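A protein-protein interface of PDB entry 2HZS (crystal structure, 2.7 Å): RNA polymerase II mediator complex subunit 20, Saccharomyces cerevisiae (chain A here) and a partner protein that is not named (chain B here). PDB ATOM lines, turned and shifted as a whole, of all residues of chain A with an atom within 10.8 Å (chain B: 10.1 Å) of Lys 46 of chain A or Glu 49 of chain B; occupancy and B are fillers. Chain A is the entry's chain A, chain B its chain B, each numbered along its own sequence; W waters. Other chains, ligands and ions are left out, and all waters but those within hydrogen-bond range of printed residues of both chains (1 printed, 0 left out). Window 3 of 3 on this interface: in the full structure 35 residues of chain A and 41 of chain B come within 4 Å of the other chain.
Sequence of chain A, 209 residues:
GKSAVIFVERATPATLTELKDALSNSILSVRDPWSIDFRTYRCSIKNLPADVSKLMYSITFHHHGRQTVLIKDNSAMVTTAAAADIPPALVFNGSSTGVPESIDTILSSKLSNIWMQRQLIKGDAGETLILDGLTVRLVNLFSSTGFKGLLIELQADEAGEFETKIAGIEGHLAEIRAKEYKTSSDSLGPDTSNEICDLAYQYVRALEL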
ATOM      1  N   ARG A  42       7.358 -18.791  11.486  1.00  0.00           N
ATOM      2  CA  ARG A  42       7.379 -19.933  12.396  1.00  0.00           C
ATOM      3  C   ARG A  42       8.752 -20.031  13.049  1.00  0.00           C
ATOM      4  O   ARG A  42       9.786 -20.057  12.375  1.00  0.00           O
ATOM      5  CB  ARG A  42       7.085 -21.237  11.658  1.00  0.00           C
ATOM      6  CG  ARG A  42       6.976 -22.441  12.577  1.00  0.00           C
ATOM      7  CD  ARG A  42       6.901 -23.730  11.770  1.00  0.00           C
ATOM      8  NE  ARG A  42       7.968 -24.657  12.143  1.00  0.00           N
ATOM      9  CZ  ARG A  42       8.001 -25.354  13.279  1.00  0.00           C
ATOM     10  NH1 ARG A  42       7.017 -25.238  14.164  1.00  0.00           N
ATOM     11  NH2 ARG A  42       9.029 -26.158  13.542  1.00  0.00           N
ATOM     12  N   CYS A  43       8.750 -20.079  14.374  1.00  0.00           N
ATOM     13  CA  CYS A  43       9.976 -20.169  15.148  1.00  0.00           C
ATOM     14  C   CYS A  43      10.658 -21.526  15.011  1.00  0.00           C
ATOM     15  O   CYS A  43       9.994 -22.569  15.078  1.00  0.00           O
ATOM     16  CB  CYS A  43       9.667 -19.915  16.612  1.00  0.00           C
ATOM     17  SG  CYS A  43      11.131 -19.696  17.603  1.00  0.00           S
ATOM     18  N   SER A  44      11.983 -21.508  14.858  1.00  0.00           N
ATOM     19  CA  SER A  44      12.775 -22.731  14.698  1.00  0.00           C
ATOM     20  C   SER A  44      13.464 -23.260  15.958  1.00  0.00           C
ATOM     21  O   SER A  44      14.165 -24.274  15.916  1.00  0.00           O
ATOM     22  CB  SER A  44      13.815 -22.525  13.604  1.00  0.00           C
ATOM     23  OG  SER A  44      13.167 -22.299  12.367  1.00  0.00           O
ATOM     24  N   ILE A  45      13.268 -22.563  17.071  1.00  0.00           N
ATOM     25  CA  ILE A  45      13.836 -22.966  18.349  1.00  0.00           C
ATOM     26  C   ILE A  45      13.183 -24.295  18.713  1.00  0.00           C
ATOM     27  O   ILE A  45      11.960 -24.434  18.603  1.00  0.00           O
ATOM     28  CB  ILE A  45      13.500 -21.929  19.447  1.00  0.00           C
ATOM     29  CG1 ILE A  45      14.048 -20.557  19.057  1.00  0.00           C
ATOM     30  CG2 ILE A  45      14.048 -22.382  20.781  1.00  0.00           C
ATOM     31  CD1 ILE A  45      15.477 -20.575  18.571  1.00  0.00           C
ATOM     32  N   LYS A  46      13.973 -25.270  19.152  1.00  0.00           N
ATOM     33  CA  LYS A  46      13.409 -26.568  19.487  1.00  0.00           C
ATOM     34  C   LYS A  46      13.226 -26.837  20.971  1.00  0.00           C
ATOM     35  O   LYS A  46      12.753 -27.912  21.336  1.00  0.00           O
ATOM     36  CB  LYS A  46      14.263 -27.691  18.890  1.00  0.00           C
ATOM     37  CG  LYS A  46      15.166 -27.263  17.751  1.00  0.00           C
ATOM     38  CD  LYS A  46      16.088 -28.402  17.334  1.00  0.00           C
ATOM     39  CE  LYS A  46      17.216 -27.917  16.418  1.00  0.00           C
ATOM     40  NZ  LYS A  46      18.188 -29.004  16.075  1.00  0.00           N
ATOM     41  N   ASN A  47      13.611 -25.891  21.826  1.00  0.00           N
ATOM     42  CA  ASN A  47      13.460 -26.070  23.282  1.00  0.00           C
ATOM     43  C   ASN A  47      12.322 -25.183  23.743  1.00  0.00           C
ATOM     44  O   ASN A  47      12.004 -25.155  24.920  1.00  0.00           O
ATOM     45  CB  ASN A  47      14.684 -25.603  24.072  1.00  0.00           C
ATOM     46  CG  ASN A  47      15.975 -25.851  23.357  1.00  0.00           C
ATOM     47  OD1 ASN A  47      16.993 -25.239  23.678  1.00  0.00           O
ATOM     48  ND2 ASN A  47      15.954 -26.759  22.376  1.00  0.00           N
ATOM     49  N   LEU A  48      11.743 -24.435  22.812  1.00  0.00           N
ATOM     50  CA  LEU A  48      10.663 -23.530  23.115  1.00  0.00           C
ATOM     51  C   LEU A  48       9.890 -23.923  24.379  1.00  0.00           C
ATOM     52  O   LEU A  48       9.223 -24.970  24.441  1.00  0.00           O
ATOM     53  CB  LEU A  48       9.711 -23.420  21.910  1.00  0.00           C
ATOM     54  CG  LEU A  48       9.643 -22.058  21.231  1.00  0.00           C
ATOM     55  CD1 LEU A  48      10.690 -21.085  21.783  1.00  0.00           C
ATOM     56  CD2 LEU A  48       9.852 -22.237  19.747  1.00  0.00           C
ATOM     57  N   PRO A  49       9.990 -23.086  25.427  1.00  0.00           N
ATOM     58  CA  PRO A  49       9.302 -23.337  26.692  1.00  0.00           C
ATOM     59  C   PRO A  49       7.836 -23.600  26.403  1.00  0.00           C
ATOM     60  O   PRO A  49       7.230 -22.911  25.562  1.00  0.00           O
ATOM     61  CB  PRO A  49       9.530 -22.036  27.471  1.00  0.00           C
ATOM     62  CG  PRO A  49      10.841 -21.560  26.938  1.00  0.00           C
ATOM     63  CD  PRO A  49      10.620 -21.758  25.467  1.00  0.00           C
ATOM     64  N   ALA A  50       7.262 -24.603  27.061  1.00  0.00           N
ATOM     65  CA  ALA A  50       5.854 -24.920  26.819  1.00  0.00           C
ATOM     66  C   ALA A  50       5.014 -23.645  26.840  1.00  0.00           C
ATOM     67  O   ALA A  50       5.337 -22.675  27.540  1.00  0.00           O
ATOM     68  CB  ALA A  50       5.359 -25.912  27.863  1.00  0.00           C
ATOM     69  N   VAL A  52       4.395 -21.072  24.629  1.00  0.00           N
ATOM     70  CA  VAL A  52       5.047 -19.910  24.114  1.00  0.00           C
ATOM     71  C   VAL A  52       4.770 -20.297  22.666  1.00  0.00           C
ATOM     72  O   VAL A  52       5.048 -21.434  22.274  1.00  0.00           O
ATOM     73  CB  VAL A  52       6.602 -19.898  24.395  1.00  0.00           C
ATOM     74  CG1 VAL A  52       7.300 -20.943  23.530  1.00  0.00           C
ATOM     75  CG2 VAL A  52       7.181 -18.518  24.146  1.00  0.00           C
ATOM     76  N   SER A  53       4.126 -19.425  21.899  1.00  0.00           N
ATOM     77  CA  SER A  53       3.809 -19.797  20.518  1.00  0.00           C
ATOM     78  C   SER A  53       5.093 -19.974  19.746  1.00  0.00           C
ATOM     79  O   SER A  53       6.178 -19.607  20.207  1.00  0.00           O
ATOM     80  CB  SER A  53       2.962 -18.706  19.871  1.00  0.00           C
ATOM     81  OG  SER A  53       1.901 -18.305  20.704  1.00  0.00           O
ATOM     82  N   LYS A  54       4.967 -20.551  18.568  1.00  0.00           N
ATOM     83  CA  LYS A  54       6.108 -20.745  17.671  1.00  0.00           C
ATOM     84  C   LYS A  54       5.755 -19.842  16.493  1.00  0.00           C
ATOM     85  O   LYS A  54       6.509 -19.730  15.520  1.00  0.00           O
ATOM     86  CB  LYS A  54       6.152 -22.198  17.192  1.00  0.00           C
ATOM     87  CG  LYS A  54       5.797 -23.212  18.268  1.00  0.00           C
ATOM     88  CD  LYS A  54       6.987 -23.586  19.137  1.00  0.00           C
ATOM     89  CE  LYS A  54       7.836 -24.657  18.466  1.00  0.00           C
ATOM     90  NZ  LYS A  54       7.076 -25.921  18.310  1.00  0.00           N
ATOM     91  N   LYS A 110      18.752 -11.488   8.505  1.00  0.00           N
ATOM     92  CA  LYS A 110      19.642 -11.591   9.647  1.00  0.00           C
ATOM     93  C   LYS A 110      19.191 -12.583  10.707  1.00  0.00           C
ATOM     94  O   LYS A 110      20.019 -13.091  11.460  1.00  0.00           O
ATOM     95  CB  LYS A 110      19.826 -10.223  10.286  1.00  0.00           C
ATOM     96  CG  LYS A 110      20.460  -9.205   9.363  1.00  0.00           C
ATOM     97  CD  LYS A 110      21.842  -9.664   8.921  1.00  0.00           C
ATOM     98  CE  LYS A 110      22.377  -8.810   7.789  1.00  0.00           C
ATOM     99  NZ  LYS A 110      23.631  -9.384   7.241  1.00  0.00           N
ATOM    100  N   LEU A 111      17.893 -12.868  10.772  1.00  0.00           N
ATOM    101  CA  LEU A 111      17.367 -13.800  11.770  1.00  0.00           C
ATOM    102  C   LEU A 111      16.649 -15.003  11.156  1.00  0.00           C
ATOM    103  O   LEU A 111      15.900 -15.701  11.840  1.00  0.00           O
ATOM    104  CB  LEU A 111      16.412 -13.062  12.711  1.00  0.00           C
ATOM    105  CG  LEU A 111      16.924 -11.757  13.329  1.00  0.00           C
ATOM    106  CD1 LEU A 111      15.854 -11.168  14.211  1.00  0.00           C
ATOM    107  CD2 LEU A 111      18.182 -12.006  14.127  1.00  0.00           C
ATOM    108  N   SER A 112      16.902 -15.254   9.875  1.00  0.00           N
ATOM    109  CA  SER A 112      16.262 -16.351   9.148  1.00  0.00           C
ATOM    110  C   SER A 112      16.418 -17.748   9.756  1.00  0.00           C
ATOM    111  O   SER A 112      15.578 -18.625   9.537  1.00  0.00           O
ATOM    112  CB  SER A 112      16.754 -16.374   7.704  1.00  0.00           C
ATOM    113  OG  SER A 112      18.162 -16.287   7.668  1.00  0.00           O
ATOM    114  N   ASN A 113      17.483 -17.967  10.512  1.00  0.00           N
ATOM    115  CA  ASN A 113      17.686 -19.266  11.117  1.00  0.00           C
ATOM    116  C   ASN A 113      16.694 -19.459  12.258  1.00  0.00           C
ATOM    117  O   ASN A 113      16.251 -20.578  12.529  1.00  0.00           O
ATOM    118  CB  ASN A 113      19.111 -19.380  11.650  1.00  0.00           C
ATOM    119  CG  ASN A 113      19.364 -18.459  12.807  1.00  0.00           C
ATOM    120  OD1 ASN A 113      19.147 -17.257  12.706  1.00  0.00           O
ATOM    121  ND2 ASN A 113      19.827 -19.014  13.922  1.00  0.00           N
ATOM    122  N   ILE A 114      16.342 -18.364  12.921  1.00  0.00           N
ATOM    123  CA  ILE A 114      15.412 -18.417  14.037  1.00  0.00           C
ATOM    124  C   ILE A 114      13.968 -18.277  13.567  1.00  0.00           C
ATOM    125  O   ILE A 114      13.065 -18.922  14.102  1.00  0.00           O
ATOM    126  CB  ILE A 114      15.721 -17.309  15.070  1.00  0.00           C
ATOM    127  CG1 ILE A 114      17.158 -17.451  15.566  1.00  0.00           C
ATOM    128  CG2 ILE A 114      14.769 -17.401  16.242  1.00  0.00           C
ATOM    129  CD1 ILE A 114      17.530 -16.445  16.603  1.00  0.00           C
ATOM    130  N   TRP A 115      13.743 -17.437  12.567  1.00  0.00           N
ATOM    131  CA  TRP A 115      12.396 -17.241  12.051  1.00  0.00           C
ATOM    132  C   TRP A 115      12.280 -17.510  10.553  1.00  0.00           C
ATOM    133  O   TRP A 115      13.020 -16.934   9.739  1.00  0.00           O
ATOM    134  CB  TRP A 115      11.922 -15.822  12.342  1.00  0.00           C
ATOM    135  CG  TRP A 115      11.856 -15.517  13.781  1.00  0.00           C
ATOM    136  CD1 TRP A 115      12.789 -14.874  14.522  1.00  0.00           C
ATOM    137  CD2 TRP A 115      10.785 -15.836  14.670  1.00  0.00           C
ATOM    138  NE1 TRP A 115      12.372 -14.766  15.824  1.00  0.00           N
ATOM    139  CE2 TRP A 115      11.146 -15.355  15.943  1.00  0.00           C
ATOM    140  CE3 TRP A 115       9.559 -16.491  14.517  1.00  0.00           C
ATOM    141  CZ2 TRP A 115      10.319 -15.494  17.056  1.00  0.00           C
ATOM    142  CZ3 TRP A 115       8.737 -16.628  15.624  1.00  0.00           C
ATOM    143  CH2 TRP A 115       9.124 -16.138  16.877  1.00  0.00           C
ATOM    144  N   MET A 116      11.338 -18.380  10.198  1.00  0.00           N
ATOM    145  CA  MET A 116      11.122 -18.726   8.801  1.00  0.00           C
ATOM    146  C   MET A 116       9.759 -18.252   8.317  1.00  0.00           C
ATOM    147  O   MET A 116       8.728 -18.523   8.943  1.00  0.00           O
ATOM    148  CB  MET A 116      11.246 -20.236   8.610  1.00  0.00           C
ATOM    149  CG  MET A 116      12.570 -20.813   9.080  1.00  0.00           C
ATOM    150  SD  MET A 116      12.702 -22.572   8.738  1.00  0.00           S
ATOM    151  CE  MET A 116      11.312 -23.223   9.792  1.00  0.00           C
ATOM    152  N   PRO B  42      21.327 -14.021  20.950  1.00  0.00           N
ATOM    153  CA  PRO B  42      20.380 -15.137  20.917  1.00  0.00           C
ATOM    154  C   PRO B  42      20.410 -15.824  22.272  1.00  0.00           C
ATOM    155  O   PRO B  42      21.482 -16.001  22.841  1.00  0.00           O
ATOM    156  CB  PRO B  42      20.934 -16.023  19.814  1.00  0.00           C
ATOM    157  CG  PRO B  42      21.613 -15.033  18.886  1.00  0.00           C
ATOM    158  CD  PRO B  42      22.305 -14.113  19.851  1.00  0.00           C
ATOM    159  N   ASN B  43      19.245 -16.201  22.797  1.00  0.00           N
ATOM    160  CA  ASN B  43      19.177 -16.868  24.100  1.00  0.00           C
ATOM    161  C   ASN B  43      20.035 -18.125  24.146  1.00  0.00           C
ATOM    162  O   ASN B  43      19.850 -19.032  23.355  1.00  0.00           O
ATOM    163  CB  ASN B  43      17.744 -17.275  24.446  1.00  0.00           C
ATOM    164  CG  ASN B  43      17.626 -17.807  25.869  1.00  0.00           C
ATOM    165  OD1 ASN B  43      18.541 -18.451  26.380  1.00  0.00           O
ATOM    166  ND2 ASN B  43      16.501 -17.537  26.512  1.00  0.00           N
ATOM    167  N   PRO B  44      20.994 -18.195  25.072  1.00  0.00           N
ATOM    168  CA  PRO B  44      21.768 -19.436  25.046  1.00  0.00           C
ATOM    169  C   PRO B  44      20.974 -20.688  25.498  1.00  0.00           C
ATOM    170  O   PRO B  44      21.269 -21.795  25.055  1.00  0.00           O
ATOM    171  CB  PRO B  44      22.981 -19.096  25.915  1.00  0.00           C
ATOM    172  CG  PRO B  44      22.480 -18.025  26.818  1.00  0.00           C
ATOM    173  CD  PRO B  44      21.645 -17.181  25.918  1.00  0.00           C
ATOM    174  N   SER B  45      19.962 -20.506  26.347  1.00  0.00           N
ATOM    175  CA  SER B  45      19.119 -21.618  26.812  1.00  0.00           C
ATOM    176  C   SER B  45      18.367 -22.264  25.656  1.00  0.00           C
ATOM    177  O   SER B  45      18.046 -23.449  25.698  1.00  0.00           O
ATOM    178  CB  SER B  45      18.075 -21.139  27.823  1.00  0.00           C
ATOM    179  OG  SER B  45      18.640 -20.827  29.085  1.00  0.00           O
ATOM    180  N   TYR B  46      18.031 -21.473  24.644  1.00  0.00           N
ATOM    181  CA  TYR B  46      17.328 -22.008  23.488  1.00  0.00           C
ATOM    182  C   TYR B  46      18.400 -22.354  22.500  1.00  0.00           C
ATOM    183  O   TYR B  46      19.440 -21.721  22.474  1.00  0.00           O
ATOM    184  CB  TYR B  46      16.472 -20.963  22.776  1.00  0.00           C
ATOM    185  CG  TYR B  46      15.411 -20.247  23.567  1.00  0.00           C
ATOM    186  CD1 TYR B  46      14.723 -20.877  24.597  1.00  0.00           C
ATOM    187  CD2 TYR B  46      15.025 -18.954  23.206  1.00  0.00           C
ATOM    188  CE1 TYR B  46      13.672 -20.243  25.243  1.00  0.00           C
ATOM    189  CE2 TYR B  46      13.979 -18.317  23.841  1.00  0.00           C
ATOM    190  CZ  TYR B  46      13.305 -18.967  24.860  1.00  0.00           C
ATOM    191  OH  TYR B  46      12.253 -18.340  25.484  1.00  0.00           O
ATOM    192  N   ASP B  47      18.183 -23.361  21.680  1.00  0.00           N
ATOM    193  CA  ASP B  47      19.189 -23.583  20.680  1.00  0.00           C
ATOM    194  C   ASP B  47      18.524 -23.997  19.410  1.00  0.00           C
ATOM    195  O   ASP B  47      17.612 -24.824  19.389  1.00  0.00           O
ATOM    196  CB  ASP B  47      20.259 -24.579  21.108  1.00  0.00           C
ATOM    197  CG  ASP B  47      21.627 -24.210  20.537  1.00  0.00           C
ATOM    198  OD1 ASP B  47      22.075 -23.058  20.769  1.00  0.00           O
ATOM    199  OD2 ASP B  47      22.241 -25.057  19.849  1.00  0.00           O
ATOM    200  N   VAL B  48      18.983 -23.363  18.350  1.00  0.00           N
ATOM    201  CA  VAL B  48      18.451 -23.582  17.034  1.00  0.00           C
ATOM    202  C   VAL B  48      19.608 -23.872  16.104  1.00  0.00           C
ATOM    203  O   VAL B  48      20.753 -23.533  16.400  1.00  0.00           O
ATOM    204  CB  VAL B  48      17.693 -22.313  16.576  1.00  0.00           C
ATOM    205  CG1 VAL B  48      18.574 -21.085  16.799  1.00  0.00           C
ATOM    206  CG2 VAL B  48      17.281 -22.438  15.115  1.00  0.00           C
ATOM    207  N   GLU B  49      19.315 -24.519  14.988  1.00  0.00           N
ATOM    208  CA  GLU B  49      20.352 -24.822  14.026  1.00  0.00           C
ATOM    209  C   GLU B  49      20.716 -23.470  13.451  1.00  0.00           C
ATOM    210  O   GLU B  49      20.005 -22.494  13.662  1.00  0.00           O
ATOM    211  CB  GLU B  49      19.808 -25.759  12.946  1.00  0.00           C
ATOM    212  CG  GLU B  49      19.148 -27.005  13.529  1.00  0.00           C
ATOM    213  CD  GLU B  49      18.366 -27.797  12.502  1.00  0.00           C
ATOM    214  OE1 GLU B  49      17.519 -27.191  11.802  1.00  0.00           O
ATOM    215  OE2 GLU B  49      18.591 -29.025  12.407  1.00  0.00           O
ATOM    216  N   ASN B  50      21.833 -23.394  12.751  1.00  0.00           N
ATOM    217  CA  ASN B  50      22.238 -22.127  12.189  1.00  0.00           C
ATOM    218  C   ASN B  50      22.076 -22.201  10.682  1.00  0.00           C
ATOM    219  O   ASN B  50      23.024 -21.990   9.926  1.00  0.00           O
ATOM    220  CB  ASN B  50      23.688 -21.826  12.595  1.00  0.00           C
ATOM    221  CG  ASN B  50      23.822 -21.408  14.077  1.00  0.00           C
ATOM    222  OD1 ASN B  50      22.993 -21.761  14.926  1.00  0.00           O
ATOM    223  ND2 ASN B  50      24.878 -20.660  14.384  1.00  0.00           N
ATOM    224  N   VAL B  51      20.855 -22.493  10.242  1.00  0.00           N
ATOM    225  CA  VAL B  51      20.611 -22.599   8.814  1.00  0.00           C
ATOM    226  C   VAL B  51      19.249 -22.105   8.345  1.00  0.00           C
ATOM    227  O   VAL B  51      18.297 -22.034   9.114  1.00  0.00           O
ATOM    228  CB  VAL B  51      20.809 -24.051   8.350  1.00  0.00           C
ATOM    229  CG1 VAL B  51      19.503 -24.821   8.416  1.00  0.00           C
ATOM    230  CG2 VAL B  51      21.389 -24.059   6.975  1.00  0.00           C
ATOM    231  N   ASN B  52      19.180 -21.771   7.062  1.00  0.00           N
ATOM    232  CA  ASN B  52      17.959 -21.281   6.419  1.00  0.00           C
ATOM    233  C   ASN B  52      16.878 -22.331   6.255  1.00  0.00           C
ATOM    234  O   ASN B  52      17.038 -23.489   6.636  1.00  0.00           O
ATOM    235  CB  ASN B  52      18.265 -20.774   5.005  1.00  0.00           C
ATOM    236  CG  ASN B  52      18.477 -19.295   4.952  1.00  0.00           C
ATOM    237  OD1 ASN B  52      17.889 -18.550   5.732  1.00  0.00           O
ATOM    238  ND2 ASN B  52      19.303 -18.847   4.014  1.00  0.00           N
ATOM    239  N   SER B  53      15.777 -21.890   5.654  1.00  0.00           N
ATOM    240  CA  SER B  53      14.656 -22.753   5.322  1.00  0.00           C
ATOM    241  C   SER B  53      15.134 -23.338   3.996  1.00  0.00           C
ATOM    242  O   SER B  53      14.633 -24.352   3.514  1.00  0.00           O
ATOM    243  CB  SER B  53      13.399 -21.924   5.085  1.00  0.00           C
ATOM    244  OG  SER B  53      13.575 -21.089   3.955  1.00  0.00           O
ATOM    245  N   ARG B  54      16.122 -22.661   3.418  1.00  0.00           N
ATOM    246  CA  ARG B  54      16.732 -23.067   2.167  1.00  0.00           C
ATOM    247  C   ARG B  54      18.012 -23.814   2.515  1.00  0.00           C
ATOM    248  O   ARG B  54      18.813 -24.125   1.636  1.00  0.00           O
ATOM    249  CB  ARG B  54      17.079 -21.842   1.325  1.00  0.00           C
ATOM    250  CG  ARG B  54      15.932 -20.864   1.113  1.00  0.00           C
ATOM    251  CD  ARG B  54      16.415 -19.435   1.382  1.00  0.00           C
ATOM    252  NE  ARG B  54      15.564 -18.404   0.793  1.00  0.00           N
ATOM    253  CZ  ARG B  54      15.740 -17.097   0.975  1.00  0.00           C
ATOM    254  NH1 ARG B  54      16.737 -16.660   1.737  1.00  0.00           N
ATOM    255  NH2 ARG B  54      14.928 -16.224   0.385  1.00  0.00           N
ATOM    256  N   ASN B  55      18.200 -24.075   3.809  1.00  0.00           N
ATOM    257  CA  ASN B  55      19.368 -24.796   4.327  1.00  0.00           C
ATOM    258  C   ASN B  55      20.693 -24.070   4.068  1.00  0.00           C
ATOM    259  O   ASN B  55      21.737 -24.699   3.850  1.00  0.00           O
ATOM    260  CB  ASN B  55      19.413 -26.213   3.736  1.00  0.00           C
ATOM    261  CG  ASN B  55      20.286 -27.167   4.543  1.00  0.00           C
ATOM    262  OD1 ASN B  55      20.156 -27.270   5.769  1.00  0.00           O
ATOM    263  ND2 ASN B  55      21.170 -27.885   3.851  1.00  0.00           N
ATOM    264  N   GLN B  56      20.639 -22.742   4.109  1.00  0.00           N
ATOM    265  CA  GLN B  56      21.818 -21.905   3.915  1.00  0.00           C
ATOM    266  C   GLN B  56      22.332 -21.380   5.260  1.00  0.00           C
ATOM    267  O   GLN B  56      21.551 -20.978   6.127  1.00  0.00           O
ATOM    268  CB  GLN B  56      21.490 -20.741   2.984  1.00  0.00           C
ATOM    269  CG  GLN B  56      21.331 -21.160   1.538  1.00  0.00           C
ATOM    270  CD  GLN B  56      20.735 -20.066   0.672  1.00  0.00           C
ATOM    271  OE1 GLN B  56      20.674 -20.195  -0.554  1.00  0.00           O
ATOM    272  NE2 GLN B  56      20.282 -18.983   1.307  1.00  0.00           N
ATOM    273  N   LEU B  57      23.651 -21.400   5.425  1.00  0.00           N
ATOM    274  CA  LEU B  57      24.284 -20.950   6.653  1.00  0.00           C
ATOM    275  C   LEU B  57      23.953 -19.525   7.038  1.00  0.00           C
ATOM    276  O   LEU B  57      24.078 -18.599   6.234  1.00  0.00           O
ATOM    277  CB  LEU B  57      25.797 -21.071   6.545  1.00  0.00           C
ATOM    278  CG  LEU B  57      26.353 -22.484   6.505  1.00  0.00           C
ATOM    279  CD1 LEU B  57      27.864 -22.388   6.365  1.00  0.00           C
ATOM    280  CD2 LEU B  57      25.954 -23.248   7.767  1.00  0.00           C
ATOM    281  N   VAL B  58      23.538 -19.367   8.289  1.00  0.00           N
ATOM    282  CA  VAL B  58      23.208 -18.067   8.858  1.00  0.00           C
ATOM    283  C   VAL B  58      24.105 -17.934  10.085  1.00  0.00           C
ATOM    284  O   VAL B  58      24.213 -18.866  10.886  1.00  0.00           O
ATOM    285  CB  VAL B  58      21.734 -18.004   9.306  1.00  0.00           C
ATOM    286  CG1 VAL B  58      21.414 -16.624   9.842  1.00  0.00           C
ATOM    287  CG2 VAL B  58      20.822 -18.356   8.149  1.00  0.00           C
ATOM    288  N   GLU B  59      24.759 -16.789  10.231  1.00  0.00           N
ATOM    289  CA  GLU B  59      25.650 -16.579  11.369  1.00  0.00           C
ATOM    290  C   GLU B  59      24.899 -15.858  12.480  1.00  0.00           C
ATOM    291  O   GLU B  59      24.197 -14.885  12.218  1.00  0.00           O
ATOM    292  CB  GLU B  59      26.851 -15.747  10.921  1.00  0.00           C
ATOM    293  CG  GLU B  59      27.279 -16.017   9.485  1.00  0.00           C
ATOM    294  CD  GLU B  59      28.618 -15.391   9.138  1.00  0.00           C
ATOM    295  OE1 GLU B  59      29.658 -15.979   9.501  1.00  0.00           O
ATOM    296  OE2 GLU B  59      28.633 -14.308   8.510  1.00  0.00           O
ATOM    297  N   PRO B  60      24.993 -16.348  13.728  1.00  0.00           N
ATOM    298  CA  PRO B  60      24.284 -15.663  14.815  1.00  0.00           C
ATOM    299  C   PRO B  60      24.911 -14.312  15.127  1.00  0.00           C
ATOM    300  O   PRO B  60      26.124 -14.186  15.199  1.00  0.00           O
ATOM    301  CB  PRO B  60      24.378 -16.653  15.978  1.00  0.00           C
ATOM    302  CG  PRO B  60      25.591 -17.447  15.667  1.00  0.00           C
ATOM    303  CD  PRO B  60      25.491 -17.656  14.179  1.00  0.00           C
HETATM  304  O   HOH W   1      22.704 -13.339  10.453  1.00  0.00           O
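The side-chain amide oxygen (OD1) of Asn 50 of chain B sits close to the backbone carbonyl oxygen (O) of Val 48 of chain B (3.2 Å). The backbone NH (N) of Arg 42 of chain A lies within hydrogen-bond range of the backbone carbonyl oxygen (O) of Met 116 of chain A, at 2.9 Å. The side-chain amide oxygen (OD1) of Asn 43 of chain B lies within hydrogen-bond range of the backbone NH (N) of Ser 45 of chain B, at 2.5 Å.
Among the printed residues, merely in contact across the chains: Asn 47 of chain A with Tyr 46 of chain B (3.3 Å), Asn 113 of chain A with Val 48 of chain B (3.3 Å), Ser 112 of chain A with Val 58 of chain B (3.4 Å), Pro 49 of chain A with Tyr 46 of chain B (3.4 Å), Ile 45 of chain A with Tyr 46 of chain B (3.4 Å), Ile 45 of chain A with Val 48 of chain B (3.5 Å), Asn 113 of chain A with Val 51 of chain B (3.5 Å), Lys 46 of chain A with Asp 47 of chain B (3.7 Å), Ser 44 of chain A with Val 48 of chain B (3.7 Å), Asn 113 of chain A with Val 58 of chain B (3.7 Å) and Met 116 of chain A with Ser 53 of chain B (3.8 Å).
Of the 19 printed residues of chain B, 9 touch a printed residue of chain A. Printed residues of chain B that touch a printed residue of chain A: Ser 45, Tyr 46, Asp 47, Val 48, Glu 49, Val 51, Asn 52, Ser 53 and Val 58. Among the printed residues, Asp or Glu carboxylates within 4 Å of a Lys or Arg side-chain nitrogen of the other chain: Lys 46 of chain A with Glu 49 of chain B (3.7 Å).
ND2 of Asn 113 of chain A sits at hydrogen-bond distance from O of Glu 49 of chain B (3.5 Å). The side-chain amide oxygen (OD1) of Asn 47 of chain A lies close to the backbone carbonyl oxygen (O) of Ser 45 of chain B, 2.9 Å away. NZ of Lys 46 of chain A lies within salt-bridge range of OE2 of Glu 49 of chain B. The side-chain amide oxygen of Asn 52 of chain B lies within hydrogen-bond range of the side-chain hydroxyl of Ser 112 of chain A (3.0 Å). The backbone NH (N) of Asp 47 of chain B sits at hydrogen-bond distance from the side-chain amide oxygen (OD1) of Asn 47 of chain A (3.0 Å).
Lys 46 of chain A touches two residues of chain B. Ile 45 of chain A touches just these residues of chain B: Tyr 46 and Val 48. Of chain A, only Ser 44 (3.7 Å), Ile 45 (3.5 Å) and Asn 113 (3.3 Å) come within 4 Å of Val 48 of chain B. No residue of chain A comes within 4 Å of Asn 50 of chain B. Val 51 of chain B touches just one residue of chain A: Asn 113 (3.5 Å). Of the printed residues of chain A, Ser 45 of chain B touches Asn 47. Of the printed residues of chain A, Tyr 46 of chain B touches Ile 45, Asn 47 and Pro 49. Printed residues of chain A within 4 Å of Ser 53 of chain B: Met 116. Glu 59 of chain B touches none of the printed residues of chain A. Pro 60 of chain B touches none of the printed residues of chain A.
Water W1 lies within hydrogen-bond range of O of Glu 59 of chain B (2.8 Å) and O of Lys 110 of chain A (2.9 Å).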
